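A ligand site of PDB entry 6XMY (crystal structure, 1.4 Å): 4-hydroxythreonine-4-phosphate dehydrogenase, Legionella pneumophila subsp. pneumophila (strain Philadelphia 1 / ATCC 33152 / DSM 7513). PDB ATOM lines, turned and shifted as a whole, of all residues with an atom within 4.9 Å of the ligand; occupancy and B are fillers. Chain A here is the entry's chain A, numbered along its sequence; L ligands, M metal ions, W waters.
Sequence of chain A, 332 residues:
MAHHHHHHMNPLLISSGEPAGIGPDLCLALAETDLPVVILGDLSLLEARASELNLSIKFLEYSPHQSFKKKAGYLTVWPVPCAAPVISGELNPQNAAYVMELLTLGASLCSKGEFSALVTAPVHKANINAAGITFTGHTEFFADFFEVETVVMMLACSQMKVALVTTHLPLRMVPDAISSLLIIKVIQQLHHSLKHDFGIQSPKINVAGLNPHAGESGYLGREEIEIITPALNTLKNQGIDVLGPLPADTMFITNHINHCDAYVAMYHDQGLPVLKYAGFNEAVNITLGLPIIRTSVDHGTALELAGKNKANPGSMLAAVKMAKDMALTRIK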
ATOM      1  N   ILE A  22      -4.369 -25.498   0.861  1.00  0.00           N
ATOM      2  CA  ILE A  22      -4.310 -26.876   0.367  1.00  0.00           C
ATOM      3  C   ILE A  22      -5.655 -27.598   0.412  1.00  0.00           C
ATOM      4  O   ILE A  22      -5.729 -28.751  -0.046  1.00  0.00           O
ATOM      5  CB  ILE A  22      -3.236 -27.734   1.069  1.00  0.00           C
ATOM      6  CG1 ILE A  22      -3.469 -27.775   2.589  1.00  0.00           C
ATOM      7  CG2 ILE A  22      -1.842 -27.264   0.689  1.00  0.00           C
ATOM      8  CD1 ILE A  22      -2.613 -28.825   3.299  1.00  0.00           C
ATOM      9  N   ALA A 121     -12.104 -29.290   5.140  1.00  0.00           N
ATOM     10  CA  ALA A 121     -10.740 -28.942   4.786  1.00  0.00           C
ATOM     11  C   ALA A 121     -10.381 -27.657   5.545  1.00  0.00           C
ATOM     12  O   ALA A 121     -11.248 -26.983   6.095  1.00  0.00           O
ATOM     13  CB  ALA A 121     -10.620 -28.783   3.268  1.00  0.00           C
ATOM     14  N   PRO A 122      -9.095 -27.276   5.602  1.00  0.00           N
ATOM     15  CA  PRO A 122      -8.724 -26.182   6.510  1.00  0.00           C
ATOM     16  C   PRO A 122      -9.128 -24.816   5.975  1.00  0.00           C
ATOM     17  O   PRO A 122      -9.198 -24.586   4.773  1.00  0.00           O
ATOM     18  CB  PRO A 122      -7.195 -26.301   6.592  1.00  0.00           C
ATOM     19  CG  PRO A 122      -6.798 -26.975   5.310  1.00  0.00           C
ATOM     20  CD  PRO A 122      -7.916 -27.916   4.986  1.00  0.00           C
ATOM     21  N   VAL A 123      -9.428 -23.913   6.916  1.00  0.00           N
ATOM     22  CA  VAL A 123      -9.718 -22.511   6.616  1.00  0.00           C
ATOM     23  C   VAL A 123      -8.679 -21.638   7.309  1.00  0.00           C
ATOM     24  O   VAL A 123      -8.057 -22.031   8.302  1.00  0.00           O
ATOM     25  CB  VAL A 123     -11.141 -22.089   7.034  1.00  0.00           C
ATOM     26  CG1 VAL A 123     -12.176 -22.975   6.345  1.00  0.00           C
ATOM     27  CG2 VAL A 123     -11.303 -22.135   8.530  1.00  0.00           C
ATOM     28  N   HIS A 124      -8.481 -20.450   6.773  1.00  0.00           N
ATOM     29  CA  HIS A 124      -7.541 -19.483   7.321  1.00  0.00           C
ATOM     30  C   HIS A 124      -8.321 -18.501   8.180  1.00  0.00           C
ATOM     31  O   HIS A 124      -9.062 -17.660   7.668  1.00  0.00           O
ATOM     32  CB  HIS A 124      -6.803 -18.763   6.200  1.00  0.00           C
ATOM     33  CG  HIS A 124      -5.575 -18.077   6.664  1.00  0.00           C
ATOM     34  ND1 HIS A 124      -5.596 -16.836   7.246  1.00  0.00           N
ATOM     35  CD2 HIS A 124      -4.281 -18.483   6.670  1.00  0.00           C
ATOM     36  CE1 HIS A 124      -4.362 -16.491   7.587  1.00  0.00           C
ATOM     37  NE2 HIS A 124      -3.552 -17.471   7.237  1.00  0.00           N
ATOM     38  N   LYS A 125      -8.154 -18.603   9.496  1.00  0.00           N
ATOM     39  CA  LYS A 125      -8.969 -17.810  10.414  1.00  0.00           C
ATOM     40  C   LYS A 125      -8.706 -16.323  10.261  1.00  0.00           C
ATOM     41  O   LYS A 125      -9.651 -15.519  10.211  1.00  0.00           O
ATOM     42  CB  LYS A 125      -8.744 -18.263  11.852  1.00  0.00           C
ATOM     43  CG  LYS A 125      -9.081 -19.721  12.121  1.00  0.00           C
ATOM     44  CD  LYS A 125      -8.850 -20.041  13.584  1.00  0.00           C
ATOM     45  CE  LYS A 125      -9.053 -21.515  13.903  1.00  0.00           C
ATOM     46  NZ  LYS A 125      -8.097 -22.402  13.187  1.00  0.00           N
ATOM     47  N   ALA A 126      -7.434 -15.921  10.193  1.00  0.00           N
ATOM     48  CA  ALA A 126      -7.130 -14.495  10.099  1.00  0.00           C
ATOM     49  C   ALA A 126      -7.711 -13.872   8.833  1.00  0.00           C
ATOM     50  O   ALA A 126      -8.192 -12.738   8.875  1.00  0.00           O
ATOM     51  CB  ALA A 126      -5.623 -14.250  10.180  1.00  0.00           C
ATOM     52  N   HIS A 138     -14.206 -23.391  13.074  1.00  0.00           N
ATOM     53  CA  HIS A 138     -15.386 -24.165  12.678  1.00  0.00           C
ATOM     54  C   HIS A 138     -16.189 -24.580  13.900  1.00  0.00           C
ATOM     55  O   HIS A 138     -17.427 -24.621  13.853  1.00  0.00           O
ATOM     56  CB  HIS A 138     -14.981 -25.477  11.988  1.00  0.00           C
ATOM     57  CG  HIS A 138     -14.391 -25.334  10.607  1.00  0.00           C
ATOM     58  ND1 HIS A 138     -13.021 -25.283  10.392  1.00  0.00           N
ATOM     59  CD2 HIS A 138     -14.964 -25.356   9.388  1.00  0.00           C
ATOM     60  CE1 HIS A 138     -12.789 -25.239   9.098  1.00  0.00           C
ATOM     61  NE2 HIS A 138     -13.947 -25.277   8.456  1.00  0.00           N
ATOM     62  N   LYS A 276      -0.294 -34.110  17.910  1.00  0.00           N
ATOM     63  CA  LYS A 276       0.177 -33.944  16.550  1.00  0.00           C
ATOM     64  C   LYS A 276       1.582 -34.491  16.383  1.00  0.00           C
ATOM     65  O   LYS A 276       1.922 -35.007  15.307  1.00  0.00           O
ATOM     66  CB  LYS A 276       0.069 -32.486  16.103  1.00  0.00           C
ATOM     67  CG  LYS A 276      -1.376 -32.016  15.992  1.00  0.00           C
ATOM     68  CD  LYS A 276      -1.491 -30.648  15.339  1.00  0.00           C
ATOM     69  CE  LYS A 276      -2.914 -30.146  15.393  1.00  0.00           C
ATOM     70  NZ  LYS A 276      -3.046 -28.893  14.578  1.00  0.00           N
ATOM     71  N   PHE A 280       0.293 -36.643  13.513  1.00  0.00           N
ATOM     72  CA  PHE A 280      -0.100 -35.536  12.628  1.00  0.00           C
ATOM     73  C   PHE A 280      -0.767 -36.016  11.335  1.00  0.00           C
ATOM     74  O   PHE A 280      -1.799 -35.460  10.928  1.00  0.00           O
ATOM     75  CB  PHE A 280       1.138 -34.711  12.295  1.00  0.00           C
ATOM     76  CG  PHE A 280       0.857 -33.435  11.547  1.00  0.00           C
ATOM     77  CD1 PHE A 280       1.498 -33.165  10.357  1.00  0.00           C
ATOM     78  CD2 PHE A 280      -0.025 -32.495  12.055  1.00  0.00           C
ATOM     79  CE1 PHE A 280       1.258 -31.988   9.671  1.00  0.00           C
ATOM     80  CE2 PHE A 280      -0.264 -31.322  11.377  1.00  0.00           C
ATOM     81  CZ  PHE A 280       0.370 -31.068  10.190  1.00  0.00           C
ATOM     82  N   ASN A 281      -0.199 -37.022  10.674  1.00  0.00           N
ATOM     83  CA  ASN A 281      -0.706 -37.423   9.358  1.00  0.00           C
ATOM     84  C   ASN A 281      -1.822 -38.461   9.413  1.00  0.00           C
ATOM     85  O   ASN A 281      -2.257 -38.944   8.361  1.00  0.00           O
ATOM     86  CB  ASN A 281       0.437 -37.881   8.454  1.00  0.00           C
ATOM     87  CG  ASN A 281       1.410 -36.760   8.169  1.00  0.00           C
ATOM     88  OD1 ASN A 281       1.028 -35.681   7.721  1.00  0.00           O
ATOM     89  ND2 ASN A 281       2.685 -37.004   8.451  1.00  0.00           N
ATOM     90  N   ASN A 285      -9.764 -34.175  13.672  1.00  0.00           N
ATOM     91  CA  ASN A 285     -10.471 -33.286  14.586  1.00  0.00           C
ATOM     92  C   ASN A 285     -11.945 -33.574  14.405  1.00  0.00           C
ATOM     93  O   ASN A 285     -12.482 -33.413  13.303  1.00  0.00           O
ATOM     94  CB  ASN A 285     -10.108 -31.831  14.249  1.00  0.00           C
ATOM     95  CG  ASN A 285     -11.058 -30.803  14.858  1.00  0.00           C
ATOM     96  OD1 ASN A 285     -11.869 -31.098  15.747  1.00  0.00           O
ATOM     97  ND2 ASN A 285     -10.948 -29.567  14.367  1.00  0.00           N
ATOM     98  N   ARG A 294     -19.472 -34.069  12.195  1.00  0.00           N
ATOM     99  CA  ARG A 294     -18.509 -33.196  11.543  1.00  0.00           C
ATOM    100  C   ARG A 294     -17.107 -33.609  11.954  1.00  0.00           C
ATOM    101  O   ARG A 294     -16.780 -33.606  13.148  1.00  0.00           O
ATOM    102  CB  ARG A 294     -18.739 -31.720  11.871  1.00  0.00           C
ATOM    103  CG  ARG A 294     -17.698 -30.798  11.235  1.00  0.00           C
ATOM    104  CD  ARG A 294     -16.637 -30.378  12.244  1.00  0.00           C
ATOM    105  NE  ARG A 294     -15.500 -29.697  11.619  1.00  0.00           N
ATOM    106  CZ  ARG A 294     -14.651 -28.904  12.266  1.00  0.00           C
ATOM    107  NH1 ARG A 294     -14.827 -28.662  13.564  1.00  0.00           N
ATOM    108  NH2 ARG A 294     -13.634 -28.338  11.625  1.00  0.00           N
ATOM    109  N   SER A 296     -12.744 -33.251  10.583  1.00  0.00           N
ATOM    110  CA  SER A 296     -11.854 -32.245  10.033  1.00  0.00           C
ATOM    111  C   SER A 296     -10.440 -32.779   9.963  1.00  0.00           C
ATOM    112  O   SER A 296     -10.049 -33.653  10.744  1.00  0.00           O
ATOM    113  CB  SER A 296     -11.891 -30.996  10.912  1.00  0.00           C
ATOM    114  OG  SER A 296     -11.062 -29.981  10.388  1.00  0.00           O
ATOM    115  N   VAL A 297      -9.664 -32.194   9.044  1.00  0.00           N
ATOM    116  CA  VAL A 297      -8.225 -32.352   9.104  1.00  0.00           C
ATOM    117  C   VAL A 297      -7.706 -31.792  10.424  1.00  0.00           C
ATOM    118  O   VAL A 297      -8.352 -30.971  11.077  1.00  0.00           O
ATOM    119  CB  VAL A 297      -7.528 -31.665   7.920  1.00  0.00           C
ATOM    120  CG1 VAL A 297      -7.902 -32.352   6.615  1.00  0.00           C
ATOM    121  CG2 VAL A 297      -7.861 -30.166   7.908  1.00  0.00           C
ATOM    122  N   HIS A 299      -4.859 -30.040  10.610  1.00  0.00           N
ATOM    123  CA  HIS A 299      -3.822 -29.126  10.173  1.00  0.00           C
ATOM    124  C   HIS A 299      -4.472 -27.924   9.524  1.00  0.00           C
ATOM    125  O   HIS A 299      -5.682 -27.898   9.275  1.00  0.00           O
ATOM    126  CB  HIS A 299      -2.834 -29.803   9.217  1.00  0.00           C
ATOM    127  CG  HIS A 299      -3.473 -30.330   7.969  1.00  0.00           C
ATOM    128  ND1 HIS A 299      -3.925 -29.502   6.970  1.00  0.00           N
ATOM    129  CD2 HIS A 299      -3.733 -31.598   7.559  1.00  0.00           C
ATOM    130  CE1 HIS A 299      -4.432 -30.232   5.991  1.00  0.00           C
ATOM    131  NE2 HIS A 299      -4.330 -31.505   6.331  1.00  0.00           N
ATOM    132  N   GLY A 300      -3.653 -26.938   9.211  1.00  0.00           N
ATOM    133  CA  GLY A 300      -4.106 -25.691   8.635  1.00  0.00           C
ATOM    134  C   GLY A 300      -3.960 -25.626   7.136  1.00  0.00           C
ATOM    135  O   GLY A 300      -3.811 -26.636   6.442  1.00  0.00           O
ATOM    136  N   THR A 301      -3.967 -24.386   6.634  1.00  0.00           N
ATOM    137  CA  THR A 301      -4.094 -24.117   5.214  1.00  0.00           C
ATOM    138  C   THR A 301      -2.809 -24.363   4.435  1.00  0.00           C
ATOM    139  O   THR A 301      -2.872 -24.503   3.208  1.00  0.00           O
ATOM    140  CB  THR A 301      -4.565 -22.669   5.003  1.00  0.00           C
ATOM    141  OG1 THR A 301      -3.803 -21.770   5.817  1.00  0.00           O
ATOM    142  CG2 THR A 301      -6.023 -22.536   5.370  1.00  0.00           C
ATOM    143  N   ALA A 302      -1.659 -24.375   5.095  1.00  0.00           N
ATOM    144  CA  ALA A 302      -0.372 -24.633   4.434  1.00  0.00           C
ATOM    145  C   ALA A 302      -0.269 -23.899   3.093  1.00  0.00           C
ATOM    146  O   ALA A 302      -0.014 -24.503   2.048  1.00  0.00           O
ATOM    147  CB  ALA A 302      -0.116 -26.136   4.296  1.00  0.00           C
ATOM    148  N   GLU A 304       1.841 -22.078   1.538  1.00  0.00           N
ATOM    149  CA  GLU A 304       3.030 -22.238   0.723  1.00  0.00           C
ATOM    150  C   GLU A 304       3.068 -23.570  -0.019  1.00  0.00           C
ATOM    151  O   GLU A 304       3.853 -23.730  -0.956  1.00  0.00           O
ATOM    152  CB  GLU A 304       4.280 -22.084   1.586  1.00  0.00           C
ATOM    153  CG  GLU A 304       4.514 -23.231   2.582  1.00  0.00           C
ATOM    154  CD  GLU A 304       3.500 -23.273   3.724  1.00  0.00           C
ATOM    155  OE1 GLU A 304       2.830 -22.249   3.987  1.00  0.00           O
ATOM    156  OE2 GLU A 304       3.375 -24.348   4.356  1.00  0.00           O
ATOM    157  N   LEU A 305       2.239 -24.549   0.388  1.00  0.00           N
ATOM    158  CA  LEU A 305       2.198 -25.835  -0.297  1.00  0.00           C
ATOM    159  C   LEU A 305       1.108 -25.912  -1.342  1.00  0.00           C
ATOM    160  O   LEU A 305       1.077 -26.886  -2.112  1.00  0.00           O
ATOM    161  CB  LEU A 305       1.993 -26.977   0.704  1.00  0.00           C
ATOM    162  CG  LEU A 305       3.019 -27.112   1.828  1.00  0.00           C
ATOM    163  CD1 LEU A 305       2.776 -28.386   2.635  1.00  0.00           C
ATOM    164  CD2 LEU A 305       4.427 -27.105   1.263  1.00  0.00           C
ATOM    165  N   LYS A 310       2.900 -31.327  -2.515  1.00  0.00           N
ATOM    166  CA  LYS A 310       3.763 -31.651  -1.391  1.00  0.00           C
ATOM    167  C   LYS A 310       3.010 -32.073  -0.137  1.00  0.00           C
ATOM    168  O   LYS A 310       3.537 -32.851   0.663  1.00  0.00           O
ATOM    169  CB  LYS A 310       4.678 -30.469  -1.024  1.00  0.00           C
ATOM    170  CG  LYS A 310       5.832 -30.267  -1.989  1.00  0.00           C
ATOM    171  CD  LYS A 310       6.592 -31.571  -2.194  1.00  0.00           C
ATOM    172  CE  LYS A 310       8.006 -31.349  -2.703  1.00  0.00           C
ATOM    173  NZ  LYS A 310       8.021 -30.681  -4.035  1.00  0.00           N
ATOM    174  N   ALA A 311       1.789 -31.579   0.051  1.00  0.00           N
ATOM    175  CA  ALA A 311       1.016 -31.868   1.239  1.00  0.00           C
ATOM    176  C   ALA A 311       0.671 -33.344   1.351  1.00  0.00           C
ATOM    177  O   ALA A 311       0.433 -34.035   0.352  1.00  0.00           O
ATOM    178  CB  ALA A 311      -0.267 -31.039   1.240  1.00  0.00           C
ATOM    179  N   ASN A 312       0.610 -33.812   2.583  1.00  0.00           N
ATOM    180  CA  ASN A 312       0.256 -35.180   2.898  1.00  0.00           C
ATOM    181  C   ASN A 312      -1.258 -35.255   3.065  1.00  0.00           C
ATOM    182  O   ASN A 312      -1.809 -34.538   3.903  1.00  0.00           O
ATOM    183  CB  ASN A 312       0.941 -35.587   4.201  1.00  0.00           C
ATOM    184  CG  ASN A 312       0.862 -37.055   4.469  1.00  0.00           C
ATOM    185  OD1 ASN A 312      -0.194 -37.668   4.329  1.00  0.00           O
ATOM    186  ND2 ASN A 312       1.975 -37.656   4.866  1.00  0.00           N
HETATM  187  P1  LIG L   1      -0.636 -25.273   9.332  1.00  0.00           P
HETATM  188  O1  LIG L   1      -1.093 -24.473   8.127  1.00  0.00           O
HETATM  189  O2  LIG L   1      -0.896 -26.728   9.637  1.00  0.00           O
HETATM  190  O3  LIG L   1       1.063 -25.168   9.095  1.00  0.00           O
HETATM  191  C1  LIG L   1       1.770 -25.834  10.104  1.00  0.00           C
HETATM  192  C2  LIG L   1       2.930 -26.653   9.496  1.00  0.00           C
HETATM  193  O4  LIG L   1       2.391 -27.908   9.019  1.00  0.00           O
HETATM  194  C3  LIG L   1       3.500 -25.881   8.275  1.00  0.00           C
HETATM  195  O5  LIG L   1       4.895 -26.138   8.282  1.00  0.00           O
HETATM  196  C4  LIG L   1       2.758 -26.553   7.083  1.00  0.00           C
HETATM  197  O6  LIG L   1       3.497 -26.552   5.891  1.00  0.00           O
HETATM  198  C5  LIG L   1       2.639 -28.016   7.613  1.00  0.00           C
HETATM  199  N1  LIG L   1       1.467 -28.719   7.108  1.00  0.00           N
HETATM  200  C6  LIG L   1       0.105 -28.485   7.360  1.00  0.00           C
HETATM  201  N2  LIG L   1      -0.683 -29.352   6.743  1.00  0.00           N
HETATM  202  C7  LIG L   1       0.180 -30.198   6.059  1.00  0.00           C
HETATM  203  C8  LIG L   1      -0.038 -31.312   5.222  1.00  0.00           C
HETATM  204  N3  LIG L   1      -1.308 -31.737   4.985  1.00  0.00           N
HETATM  205  N4  LIG L   1       1.019 -31.976   4.671  1.00  0.00           N
HETATM  206  C9  LIG L   1       2.273 -31.504   4.966  1.00  0.00           C
HETATM  207  N5  LIG L   1       2.634 -30.462   5.734  1.00  0.00           N
HETATM  208  C10 LIG L   1       1.543 -29.818   6.274  1.00  0.00           C
HETATM  209  O7  LIG L   1      -1.152 -24.383  10.588  1.00  0.00           O
HETATM  210  P2  LIG L   1      -0.670 -22.950  11.067  1.00  0.00           P
HETATM  211  O8  LIG L   1      -0.698 -22.821  12.567  1.00  0.00           O
HETATM  212  O9  LIG L   1       0.361 -22.415  10.126  1.00  0.00           O
HETATM  213  O10 LIG L   1      -2.072 -21.929  10.692  1.00  0.00           O
HETATM  214  C11 LIG L   1      -2.316 -21.730   9.334  1.00  0.00           C
HETATM  215  C12 LIG L   1      -3.795 -21.370   9.199  1.00  0.00           C
HETATM  216  O11 LIG L   1      -4.560 -22.592   9.289  1.00  0.00           O
HETATM  217  C13 LIG L   1      -4.253 -20.468  10.407  1.00  0.00           C
HETATM  218  O12 LIG L   1      -5.196 -19.585   9.879  1.00  0.00           O
HETATM  219  C14 LIG L   1      -4.915 -21.485  11.351  1.00  0.00           C
HETATM  220  O13 LIG L   1      -5.960 -20.964  12.144  1.00  0.00           O
HETATM  221  C15 LIG L   1      -5.573 -22.382  10.269  1.00  0.00           C
HETATM  222  N6  LIG L   1      -5.941 -23.738  10.805  1.00  0.00           N
HETATM  223  C16 LIG L   1      -7.167 -24.216  10.428  1.00  0.00           C
HETATM  224  C17 LIG L   1      -7.591 -25.474  10.867  1.00  0.00           C
HETATM  225  C18 LIG L   1      -8.923 -25.894  10.382  1.00  0.00           C
HETATM  226  O14 LIG L   1      -9.579 -25.194   9.606  1.00  0.00           O
HETATM  227  N7  LIG L   1      -9.380 -27.119  10.826  1.00  0.00           N
HETATM  228  C19 LIG L   1      -6.762 -26.249  11.697  1.00  0.00           C
HETATM  229  C20 LIG L   1      -5.501 -25.736  12.060  1.00  0.00           C
HETATM  230  C21 LIG L   1      -5.093 -24.456  11.610  1.00  0.00           C
HETATM  231 ZN    ZN M   1      -5.856 -24.941  16.454  1.00  0.00          ZN
HETATM  232  O   HOH W   1       3.165 -22.558  10.505  1.00  0.00           O
HETATM  233  O   HOH W   2       5.958 -24.064   6.804  1.00  0.00           O
HETATM  234  O   HOH W   3      -7.199 -24.922  14.664  1.00  0.00           O
HETATM  235  O   HOH W   4       0.803 -22.859   7.035  1.00  0.00           O
HETATM  236  O   HOH W   5      -8.443 -28.995  12.855  1.00  0.00           O
HETATM  237  O   HOH W   6       0.597 -19.914  13.394  1.00  0.00           O
HETATM  238  O   HOH W   7       2.976 -33.760   6.961  1.00  0.00           O
HETATM  239  O   HOH W   8      -2.015 -27.153  12.485  1.00  0.00           O
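A ring nitrogen (ND1) of His 299 lies close to a nitrogen (N2) of the ligand, 3.3 Å away.
A nitrogen (N4) of the ligand is in hydrogen-bond range of the backbone NH (N) of Asn 312, 2.8 Å away.
The side-chain hydroxyl (OG) of Ser 296 lies within hydrogen-bond range of a nitrogen (N7) of the ligand (3.3 Å).
An oxygen (O2) of the ligand sits at hydrogen-bond distance from the backbone NH (N) of Gly 300 (2.8 Å).
The backbone NH of Val 123 is in hydrogen-bond range of an oxygen (O14) of the ligand (3.0 Å).
O1 of the ligand lies within hydrogen-bond range of N of Thr 301 (3.2 Å).
OE2 of Glu 304 lies within hydrogen-bond range of O6 of the ligand, at 2.7 Å.
NZ of Lys 125 is in hydrogen-bond range of O13 of the ligand (2.8 Å).
O1 of the ligand is in hydrogen-bond range of N of Ala 302.
The backbone NH (N) of Lys 125 sits at hydrogen-bond distance from an oxygen (O12) of the ligand (3.1 Å).
The backbone carbonyl oxygen of Asn 312 is in hydrogen-bond range of a nitrogen (N3) of the ligand (3.0 Å).
A ring nitrogen (ND1) of His 138 sits close to the guanidinium group of Arg 294, at 3.4 Å.
The backbone NH (N) of Ser 296 sits at hydrogen-bond distance from the backbone carbonyl oxygen (O) of Asn 285, 2.7 Å away.
The backbone NH of Ile 22 lies within hydrogen-bond range of the backbone carbonyl oxygen of Thr 301, 3.0 Å away.
The side-chain hydroxyl (OG) of Ser 296 lies close to the guanidinium group (NH2) of Arg 294, 3.3 Å away.
Merely in contact with the ligand: His 138 (3.3 Å), Pro 122 (3.4 Å), Ala 311 (3.4 Å), His 124 (3.5 Å), Ile 22 (3.6 Å), Leu 305 (3.7 Å), Phe 280 (3.8 Å) and Val 297 (3.99 Å).
Hydrophobic or aromatic side chains within 4 Å of the ligand: Ile 22, Pro 122, Val 123, His 124, His 138, Phe 280, His 299, Ala 302, Leu 305 and Ala 311.
Within 4 Å of the ligand: Ile 22, Pro 122, Val 123, His 124, Lys 125, His 138, Phe 280, Ser 296, Val 297, His 299, Gly 300, Thr 301, Ala 302, Glu 304, Leu 305, Ala 311 and Asn 312.
Along chain A the residues within 4 Å of the ligand span positions 22 to 312.
Water W4 lies within hydrogen-bond range of an oxygen (O1) of the ligand and the backbone NH of Ala 302.
Water W5 lies within hydrogen-bond range of the backbone carbonyl oxygen (O) of Val 297, a nitrogen (N7) of the ligand and the side-chain amide nitrogen (ND2) of Asn 285.
Water W8 bridges the side-chain amino group of Lys 276 and an oxygen (O2) of the ligand.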
